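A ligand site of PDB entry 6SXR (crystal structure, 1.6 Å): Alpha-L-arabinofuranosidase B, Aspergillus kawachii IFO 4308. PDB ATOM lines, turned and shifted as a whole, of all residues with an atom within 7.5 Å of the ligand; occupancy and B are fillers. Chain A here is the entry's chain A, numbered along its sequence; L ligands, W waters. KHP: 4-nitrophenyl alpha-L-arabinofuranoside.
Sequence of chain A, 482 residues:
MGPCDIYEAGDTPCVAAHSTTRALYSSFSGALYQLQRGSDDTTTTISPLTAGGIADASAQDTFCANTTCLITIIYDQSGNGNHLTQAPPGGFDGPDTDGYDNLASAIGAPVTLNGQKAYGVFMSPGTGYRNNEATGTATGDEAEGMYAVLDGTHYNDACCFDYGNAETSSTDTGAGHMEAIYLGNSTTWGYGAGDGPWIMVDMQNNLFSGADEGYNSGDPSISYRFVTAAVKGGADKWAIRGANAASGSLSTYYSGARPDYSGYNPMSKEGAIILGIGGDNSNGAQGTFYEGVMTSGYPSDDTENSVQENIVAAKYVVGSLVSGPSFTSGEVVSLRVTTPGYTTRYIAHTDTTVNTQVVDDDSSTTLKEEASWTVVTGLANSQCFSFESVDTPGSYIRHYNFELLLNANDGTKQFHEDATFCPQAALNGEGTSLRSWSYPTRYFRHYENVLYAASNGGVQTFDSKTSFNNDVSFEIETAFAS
O of Asp 471 lies within hydrogen-bond range of N of His 446, 3.2 Å away. The side-chain carboxylate of Asp 471 lies within hydrogen-bond range of the side-chain hydroxyl of Thr 339, 2.8 Å away. The guanidinium group (NH2) of Arg 445 is in salt-bridge range of the side-chain carboxylate (OD2) of Asp 471, at 2.9 Å. A ring nitrogen (NE2) of His 446 lies within hydrogen-bond range of the side-chain hydroxyl of Thr 339 (3.0 Å). The side-chain amide nitrogen (ND2) of Asn 449 lies close to the guanidinium group (NH1) of Arg 345, 3.4 Å away. O of Thr 466 is in hydrogen-bond range of NH2 of Arg 445 (2.9 Å). The guanidinium group (NH1) of Arg 445 is in hydrogen-bond range of the backbone carbonyl oxygen (O) of Ser 464, at 2.8 Å. The backbone carbonyl oxygen (O) of Phe 462 sits at hydrogen-bond distance from the guanidinium group (NH1) of Arg 445.
Water W1 lies within hydrogen-bond range of an oxygen (O2) of the ligand and the backbone carbonyl oxygen (O) of Thr 466. Water W2 lies within hydrogen-bond range of O3 of the ligand (2.8 Å) and OG of Ser 467 (3.3 Å).
The side-chain carboxylate (OD2) of Asp 471 is in hydrogen-bond range of an oxygen (O2) of the ligand (2.6 Å). A ring nitrogen (ND1) of His 446 sits at hydrogen-bond distance from an oxygen (O5) of the ligand (2.8 Å). The backbone NH (N) of Asn 449 sits at hydrogen-bond distance from an oxygen (O5) of the ligand (2.9 Å). An oxygen (O4) of the ligand lies within hydrogen-bond range of the backbone NH (N) of Glu 448 (2.9 Å). The backbone NH of Tyr 447 sits at hydrogen-bond distance from an oxygen (O5) of the ligand, 3.5 Å away.
Residues that only touch the ligand: Tyr 342, Thr 339, Arg 445 and Ser 467. Within 4 Å of the ligand: Thr 339, Tyr 342, Arg 445, His 446, Tyr 447, Glu 448, Asn 449, Ser 467 and Asp 471.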
ATOM      1  N   VAL A 337      24.428  13.400 -18.669  1.00  0.00           N
ATOM      2  CA  VAL A 337      24.120  14.854 -18.610  1.00  0.00           C
ATOM      3  C   VAL A 337      25.220  15.547 -17.792  1.00  0.00           C
ATOM      4  O   VAL A 337      25.723  14.928 -16.818  1.00  0.00           O
ATOM      5  CB  VAL A 337      22.737  15.106 -18.039  1.00  0.00           C
ATOM      6  CG1 VAL A 337      22.514  16.561 -17.707  1.00  0.00           C
ATOM      7  CG2 VAL A 337      21.665  14.615 -18.987  1.00  0.00           C
ATOM      8  N   THR A 339      25.024  19.126 -17.189  1.00  0.00           N
ATOM      9  CA  THR A 339      24.456  20.370 -16.621  1.00  0.00           C
ATOM     10  C   THR A 339      24.340  20.267 -15.091  1.00  0.00           C
ATOM     11  O   THR A 339      23.678  19.334 -14.605  1.00  0.00           O
ATOM     12  CB  THR A 339      23.067  20.612 -17.165  1.00  0.00           C
ATOM     13  OG1 THR A 339      23.185  20.644 -18.593  1.00  0.00           O
ATOM     14  CG2 THR A 339      22.485  21.906 -16.639  1.00  0.00           C
ATOM     15  N   PRO A 340      24.923  21.232 -14.336  1.00  0.00           N
ATOM     16  CA  PRO A 340      24.805  21.275 -12.859  1.00  0.00           C
ATOM     17  C   PRO A 340      23.343  21.148 -12.446  1.00  0.00           C
ATOM     18  O   PRO A 340      22.477  21.821 -12.986  1.00  0.00           O
ATOM     19  CB  PRO A 340      25.427  22.621 -12.469  1.00  0.00           C
ATOM     20  CG  PRO A 340      26.472  22.825 -13.549  1.00  0.00           C
ATOM     21  CD  PRO A 340      25.752  22.360 -14.817  1.00  0.00           C
ATOM     22  N   GLY A 341      23.099  20.226 -11.523  1.00  0.00           N
ATOM     23  CA  GLY A 341      21.724  19.926 -11.069  1.00  0.00           C
ATOM     24  C   GLY A 341      21.150  18.681 -11.720  1.00  0.00           C
ATOM     25  O   GLY A 341      20.036  18.263 -11.318  1.00  0.00           O
ATOM     26  N   TYR A 342      21.796  18.129 -12.759  1.00  0.00           N
ATOM     27  CA  TYR A 342      21.199  17.039 -13.566  1.00  0.00           C
ATOM     28  C   TYR A 342      22.243  15.997 -13.883  1.00  0.00           C
ATOM     29  O   TYR A 342      22.014  15.152 -14.788  1.00  0.00           O
ATOM     30  CB  TYR A 342      20.530  17.651 -14.801  1.00  0.00           C
ATOM     31  CG  TYR A 342      19.497  18.706 -14.537  1.00  0.00           C
ATOM     32  CD1 TYR A 342      18.158  18.394 -14.425  1.00  0.00           C
ATOM     33  CD2 TYR A 342      19.860  20.041 -14.421  1.00  0.00           C
ATOM     34  CE1 TYR A 342      17.202  19.367 -14.206  1.00  0.00           C
ATOM     35  CE2 TYR A 342      18.925  21.024 -14.163  1.00  0.00           C
ATOM     36  CZ  TYR A 342      17.596  20.684 -14.045  1.00  0.00           C
ATOM     37  OH  TYR A 342      16.681  21.647 -13.890  1.00  0.00           O
ATOM     38  N   ARG A 345      21.759  12.173 -14.419  1.00  0.00           N
ATOM     39  CA  ARG A 345      20.817  11.767 -15.475  1.00  0.00           C
ATOM     40  C   ARG A 345      21.591  11.328 -16.729  1.00  0.00           C
ATOM     41  O   ARG A 345      22.700  11.833 -16.996  1.00  0.00           O
ATOM     42  CB  ARG A 345      19.808  12.856 -15.795  1.00  0.00           C
ATOM     43  CG  ARG A 345      19.081  13.396 -14.565  1.00  0.00           C
ATOM     44  CD  ARG A 345      18.068  14.409 -14.961  1.00  0.00           C
ATOM     45  NE  ARG A 345      16.823  13.849 -15.459  1.00  0.00           N
ATOM     46  CZ  ARG A 345      15.780  13.511 -14.684  1.00  0.00           C
ATOM     47  NH1 ARG A 345      14.665  13.042 -15.218  1.00  0.00           N
ATOM     48  NH2 ARG A 345      15.874  13.640 -13.370  1.00  0.00           N
ATOM     49  N   THR A 356      15.819  12.477 -20.420  1.00  0.00           N
ATOM     50  CA  THR A 356      16.871  12.164 -19.458  1.00  0.00           C
ATOM     51  C   THR A 356      16.216  11.564 -18.200  1.00  0.00           C
ATOM     52  O   THR A 356      15.145  12.052 -17.854  1.00  0.00           O
ATOM     53  CB  THR A 356      17.775  13.349 -19.136  1.00  0.00           C
ATOM     54  OG1 THR A 356      17.064  14.289 -18.339  1.00  0.00           O
ATOM     55  CG2 THR A 356      18.285  14.026 -20.410  1.00  0.00           C
ATOM     56  N   ARG A 445      20.012  18.342 -27.165  1.00  0.00           N
ATOM     57  CA  ARG A 445      19.875  19.359 -26.100  1.00  0.00           C
ATOM     58  C   ARG A 445      18.743  18.914 -25.173  1.00  0.00           C
ATOM     59  O   ARG A 445      17.584  18.712 -25.699  1.00  0.00           O
ATOM     60  CB  ARG A 445      19.577  20.745 -26.686  1.00  0.00           C
ATOM     61  CG  ARG A 445      19.553  21.885 -25.662  1.00  0.00           C
ATOM     62  CD  ARG A 445      18.185  22.233 -25.009  1.00  0.00           C
ATOM     63  NE  ARG A 445      18.528  23.178 -23.966  1.00  0.00           N
ATOM     64  CZ  ARG A 445      18.726  24.494 -24.147  1.00  0.00           C
ATOM     65  NH1 ARG A 445      18.370  25.090 -25.272  1.00  0.00           N
ATOM     66  NH2 ARG A 445      19.230  25.236 -23.160  1.00  0.00           N
ATOM     67  N   HIS A 446      19.050  18.778 -23.886  1.00  0.00           N
ATOM     68  CA  HIS A 446      17.959  18.490 -22.911  1.00  0.00           C
ATOM     69  C   HIS A 446      17.370  19.818 -22.399  1.00  0.00           C
ATOM     70  O   HIS A 446      18.108  20.773 -22.111  1.00  0.00           O
ATOM     71  CB  HIS A 446      18.376  17.513 -21.831  1.00  0.00           C
ATOM     72  CG  HIS A 446      19.405  18.061 -20.913  1.00  0.00           C
ATOM     73  ND1 HIS A 446      19.038  18.768 -19.806  1.00  0.00           N
ATOM     74  CD2 HIS A 446      20.754  18.048 -20.983  1.00  0.00           C
ATOM     75  CE1 HIS A 446      20.133  19.175 -19.195  1.00  0.00           C
ATOM     76  NE2 HIS A 446      21.205  18.740 -19.880  1.00  0.00           N
ATOM     77  N   TYR A 447      16.062  19.820 -22.313  1.00  0.00           N
ATOM     78  CA  TYR A 447      15.211  20.932 -21.849  1.00  0.00           C
ATOM     79  C   TYR A 447      13.992  20.311 -21.141  1.00  0.00           C
ATOM     80  O   TYR A 447      13.244  19.536 -21.746  1.00  0.00           O
ATOM     81  CB  TYR A 447      14.804  21.783 -23.043  1.00  0.00           C
ATOM     82  CG  TYR A 447      14.065  23.024 -22.642  1.00  0.00           C
ATOM     83  CD1 TYR A 447      14.738  24.184 -22.270  1.00  0.00           C
ATOM     84  CD2 TYR A 447      12.689  23.051 -22.646  1.00  0.00           C
ATOM     85  CE1 TYR A 447      14.049  25.333 -21.903  1.00  0.00           C
ATOM     86  CE2 TYR A 447      11.983  24.191 -22.291  1.00  0.00           C
ATOM     87  CZ  TYR A 447      12.674  25.319 -21.913  1.00  0.00           C
ATOM     88  OH  TYR A 447      11.928  26.413 -21.594  1.00  0.00           O
ATOM     89  N   GLU A 448      13.816  20.678 -19.877  1.00  0.00           N
ATOM     90  CA  GLU A 448      12.865  19.986 -18.943  1.00  0.00           C
ATOM     91  C   GLU A 448      12.959  18.470 -19.096  1.00  0.00           C
ATOM     92  O   GLU A 448      11.914  17.789 -19.100  1.00  0.00           O
ATOM     93  CB  GLU A 448      11.449  20.475 -19.202  1.00  0.00           C
ATOM     94  CG  GLU A 448      11.334  21.952 -18.980  1.00  0.00           C
ATOM     95  CD  GLU A 448       9.930  22.495 -19.113  1.00  0.00           C
ATOM     96  OE1 GLU A 448       9.057  21.771 -19.579  1.00  0.00           O
ATOM     97  OE2 GLU A 448       9.738  23.651 -18.765  1.00  0.00           O
ATOM     98  N   ASN A 449      14.186  17.959 -19.130  1.00  0.00           N
ATOM     99  CA  ASN A 449      14.530  16.528 -19.094  1.00  0.00           C
ATOM    100  C   ASN A 449      13.952  15.816 -20.314  1.00  0.00           C
ATOM    101  O   ASN A 449      13.876  14.577 -20.261  1.00  0.00           O
ATOM    102  CB  ASN A 449      14.047  15.873 -17.783  1.00  0.00           C
ATOM    103  CG  ASN A 449      14.674  16.475 -16.547  1.00  0.00           C
ATOM    104  OD1 ASN A 449      15.794  16.981 -16.586  1.00  0.00           O
ATOM    105  ND2 ASN A 449      14.001  16.340 -15.403  1.00  0.00           N
ATOM    106  N   VAL A 450      13.737  16.527 -21.413  1.00  0.00           N
ATOM    107  CA  VAL A 450      13.358  15.945 -22.723  1.00  0.00           C
ATOM    108  C   VAL A 450      14.438  16.318 -23.762  1.00  0.00           C
ATOM    109  O   VAL A 450      15.013  17.388 -23.595  1.00  0.00           O
ATOM    110  CB  VAL A 450      11.983  16.470 -23.139  1.00  0.00           C
ATOM    111  CG1 VAL A 450      11.556  15.962 -24.494  1.00  0.00           C
ATOM    112  CG2 VAL A 450      10.943  16.062 -22.091  1.00  0.00           C
ATOM    113  N   LEU A 451      14.728  15.419 -24.718  1.00  0.00           N
ATOM    114  CA  LEU A 451      15.787  15.677 -25.737  1.00  0.00           C
ATOM    115  C   LEU A 451      15.171  16.344 -26.952  1.00  0.00           C
ATOM    116  O   LEU A 451      14.141  15.888 -27.493  1.00  0.00           O
ATOM    117  CB  LEU A 451      16.550  14.417 -26.134  1.00  0.00           C
ATOM    118  CG  LEU A 451      17.831  14.141 -25.359  1.00  0.00           C
ATOM    119  CD1 LEU A 451      18.912  15.184 -25.590  1.00  0.00           C
ATOM    120  CD2 LEU A 451      17.559  14.072 -23.856  1.00  0.00           C
ATOM    121  N   THR A 461      10.772  27.134 -27.751  1.00  0.00           N
ATOM    122  CA  THR A 461      11.111  27.312 -26.318  1.00  0.00           C
ATOM    123  C   THR A 461      12.392  26.575 -25.969  1.00  0.00           C
ATOM    124  O   THR A 461      13.217  27.069 -25.176  1.00  0.00           O
ATOM    125  CB  THR A 461       9.957  26.811 -25.429  1.00  0.00           C
ATOM    126  OG1 THR A 461       8.748  27.414 -25.908  1.00  0.00           O
ATOM    127  CG2 THR A 461      10.150  27.212 -23.986  1.00  0.00           C
ATOM    128  N   PHE A 462      12.569  25.388 -26.543  1.00  0.00           N
ATOM    129  CA  PHE A 462      13.724  24.538 -26.200  1.00  0.00           C
ATOM    130  C   PHE A 462      15.017  24.990 -26.895  1.00  0.00           C
ATOM    131  O   PHE A 462      16.055  24.378 -26.640  1.00  0.00           O
ATOM    132  CB  PHE A 462      13.426  23.078 -26.531  1.00  0.00           C
ATOM    133  CG  PHE A 462      12.918  22.845 -27.922  1.00  0.00           C
ATOM    134  CD1 PHE A 462      13.806  22.733 -28.986  1.00  0.00           C
ATOM    135  CD2 PHE A 462      11.557  22.676 -28.160  1.00  0.00           C
ATOM    136  CE1 PHE A 462      13.326  22.480 -30.266  1.00  0.00           C
ATOM    137  CE2 PHE A 462      11.091  22.425 -29.436  1.00  0.00           C
ATOM    138  CZ  PHE A 462      11.985  22.303 -30.493  1.00  0.00           C
ATOM    139  N   SER A 464      16.207  27.812 -25.930  1.00  0.00           N
ATOM    140  CA  SER A 464      16.687  28.819 -24.945  1.00  0.00           C
ATOM    141  C   SER A 464      18.209  28.861 -24.871  1.00  0.00           C
ATOM    142  O   SER A 464      18.863  27.823 -24.763  1.00  0.00           O
ATOM    143  CB  SER A 464      16.127  28.578 -23.580  1.00  0.00           C
ATOM    144  OG  SER A 464      16.620  29.570 -22.682  1.00  0.00           O
ATOM    145  N   LYS A 465      18.773  30.058 -24.840  1.00  0.00           N
ATOM    146  CA  LYS A 465      20.228  30.236 -24.688  1.00  0.00           C
ATOM    147  C   LYS A 465      20.661  29.909 -23.259  1.00  0.00           C
ATOM    148  O   LYS A 465      21.837  29.582 -23.039  1.00  0.00           O
ATOM    149  CB  LYS A 465      20.607  31.680 -25.007  1.00  0.00           C
ATOM    150  CG  LYS A 465      20.204  32.082 -26.406  1.00  0.00           C
ATOM    151  CD  LYS A 465      20.907  33.348 -26.835  1.00  0.00           C
ATOM    152  CE  LYS A 465      22.132  33.071 -27.639  1.00  0.00           C
ATOM    153  NZ  LYS A 465      22.520  34.277 -28.398  1.00  0.00           N
ATOM    154  N   THR A 466      19.749  30.046 -22.300  1.00  0.00           N
ATOM    155  CA  THR A 466      20.071  29.661 -20.895  1.00  0.00           C
ATOM    156  C   THR A 466      20.487  28.206 -20.820  1.00  0.00           C
ATOM    157  O   THR A 466      19.732  27.366 -21.323  1.00  0.00           O
ATOM    158  CB  THR A 466      18.902  29.946 -19.964  1.00  0.00           C
ATOM    159  OG1 THR A 466      18.625  31.329 -20.073  1.00  0.00           O
ATOM    160  CG2 THR A 466      19.244  29.593 -18.527  1.00  0.00           C
ATOM    161  N   SER A 467      21.682  27.963 -20.289  1.00  0.00           N
ATOM    162  CA  SER A 467      22.292  26.637 -20.032  1.00  0.00           C
ATOM    163  C   SER A 467      22.551  25.891 -21.358  1.00  0.00           C
ATOM    164  O   SER A 467      22.758  24.685 -21.335  1.00  0.00           O
ATOM    165  CB  SER A 467      21.369  25.880 -19.066  1.00  0.00           C
ATOM    166  OG  SER A 467      22.085  24.862 -18.438  1.00  0.00           O
ATOM    167  N   PHE A 468      22.669  26.601 -22.486  1.00  0.00           N
ATOM    168  CA  PHE A 468      22.774  25.901 -23.789  1.00  0.00           C
ATOM    169  C   PHE A 468      24.054  25.065 -23.810  1.00  0.00           C
ATOM    170  O   PHE A 468      24.000  23.854 -24.097  1.00  0.00           O
ATOM    171  CB  PHE A 468      22.723  26.854 -24.990  1.00  0.00           C
ATOM    172  CG  PHE A 468      22.798  26.120 -26.302  1.00  0.00           C
ATOM    173  CD1 PHE A 468      21.660  25.630 -26.925  1.00  0.00           C
ATOM    174  CD2 PHE A 468      24.044  25.887 -26.881  1.00  0.00           C
ATOM    175  CE1 PHE A 468      21.749  24.963 -28.141  1.00  0.00           C
ATOM    176  CE2 PHE A 468      24.122  25.200 -28.102  1.00  0.00           C
ATOM    177  CZ  PHE A 468      22.984  24.705 -28.704  1.00  0.00           C
ATOM    178  N   ASN A 470      25.980  23.792 -21.552  1.00  0.00           N
ATOM    179  CA  ASN A 470      25.909  22.629 -20.621  1.00  0.00           C
ATOM    180  C   ASN A 470      24.912  21.588 -21.154  1.00  0.00           C
ATOM    181  O   ASN A 470      25.256  20.344 -21.151  1.00  0.00           O
ATOM    182  CB  ASN A 470      25.563  23.110 -19.205  1.00  0.00           C
ATOM    183  CG  ASN A 470      26.717  23.819 -18.531  1.00  0.00           C
ATOM    184  OD1 ASN A 470      27.865  23.599 -18.888  1.00  0.00           O
ATOM    185  ND2 ASN A 470      26.421  24.659 -17.559  1.00  0.00           N
ATOM    186  N   ASP A 471      23.775  22.044 -21.640  1.00  0.00           N
ATOM    187  CA  ASP A 471      22.604  21.204 -22.044  1.00  0.00           C
ATOM    188  C   ASP A 471      22.927  20.438 -23.329  1.00  0.00           C
ATOM    189  O   ASP A 471      22.195  19.485 -23.575  1.00  0.00           O
ATOM    190  CB  ASP A 471      21.327  22.012 -22.216  1.00  0.00           C
ATOM    191  CG  ASP A 471      20.702  22.579 -20.924  1.00  0.00           C
ATOM    192  OD1 ASP A 471      21.220  22.236 -19.801  1.00  0.00           O
ATOM    193  OD2 ASP A 471      19.771  23.370 -21.070  1.00  0.00           O
HETATM  194  O5  KHP L   1      16.538  19.619 -18.890  1.00  0.00           O
HETATM  195  C5  KHP L   1      16.884  20.131 -17.645  1.00  0.00           C
HETATM  196  C4  KHP L   1      16.843  21.626 -17.599  1.00  0.00           C
HETATM  197  O4  KHP L   1      15.646  22.114 -18.142  1.00  0.00           O
HETATM  198  C1  KHP L   1      15.885  23.478 -18.523  1.00  0.00           C
HETATM  199  C2  KHP L   1      17.378  23.668 -18.785  1.00  0.00           C
HETATM  200  O2  KHP L   1      17.468  24.117 -20.146  1.00  0.00           O
HETATM  201  C3  KHP L   1      17.919  22.291 -18.509  1.00  0.00           C
HETATM  202  O3  KHP L   1      19.214  22.303 -17.942  1.00  0.00           O
HETATM  203  O1  KHP L   1      15.605  24.379 -17.498  1.00  0.00           O
HETATM  204  C1' KHP L   1      14.308  24.634 -17.205  1.00  0.00           C
HETATM  205  C2' KHP L   1      13.879  24.378 -15.896  1.00  0.00           C
HETATM  206  C3' KHP L   1      12.563  24.601 -15.541  1.00  0.00           C
HETATM  207  C4' KHP L   1      11.716  25.103 -16.531  1.00  0.00           C
HETATM  208  N1' KHP L   1      10.379  25.340 -16.210  1.00  0.00           N
HETATM  209  O3' KHP L   1       9.718  26.419 -16.826  1.00  0.00           O
HETATM  210  O2' KHP L   1       9.824  24.575 -15.414  1.00  0.00           O
HETATM  211  C5' KHP L   1      12.144  25.358 -17.840  1.00  0.00           C
HETATM  212  C6' KHP L   1      13.461  25.130 -18.173  1.00  0.00           C
HETATM  213  O   HOH W   1      17.200  26.740 -20.627  1.00  0.00           O
HETATM  214  O   HOH W   2      19.729  24.359 -16.148  1.00  0.00           O
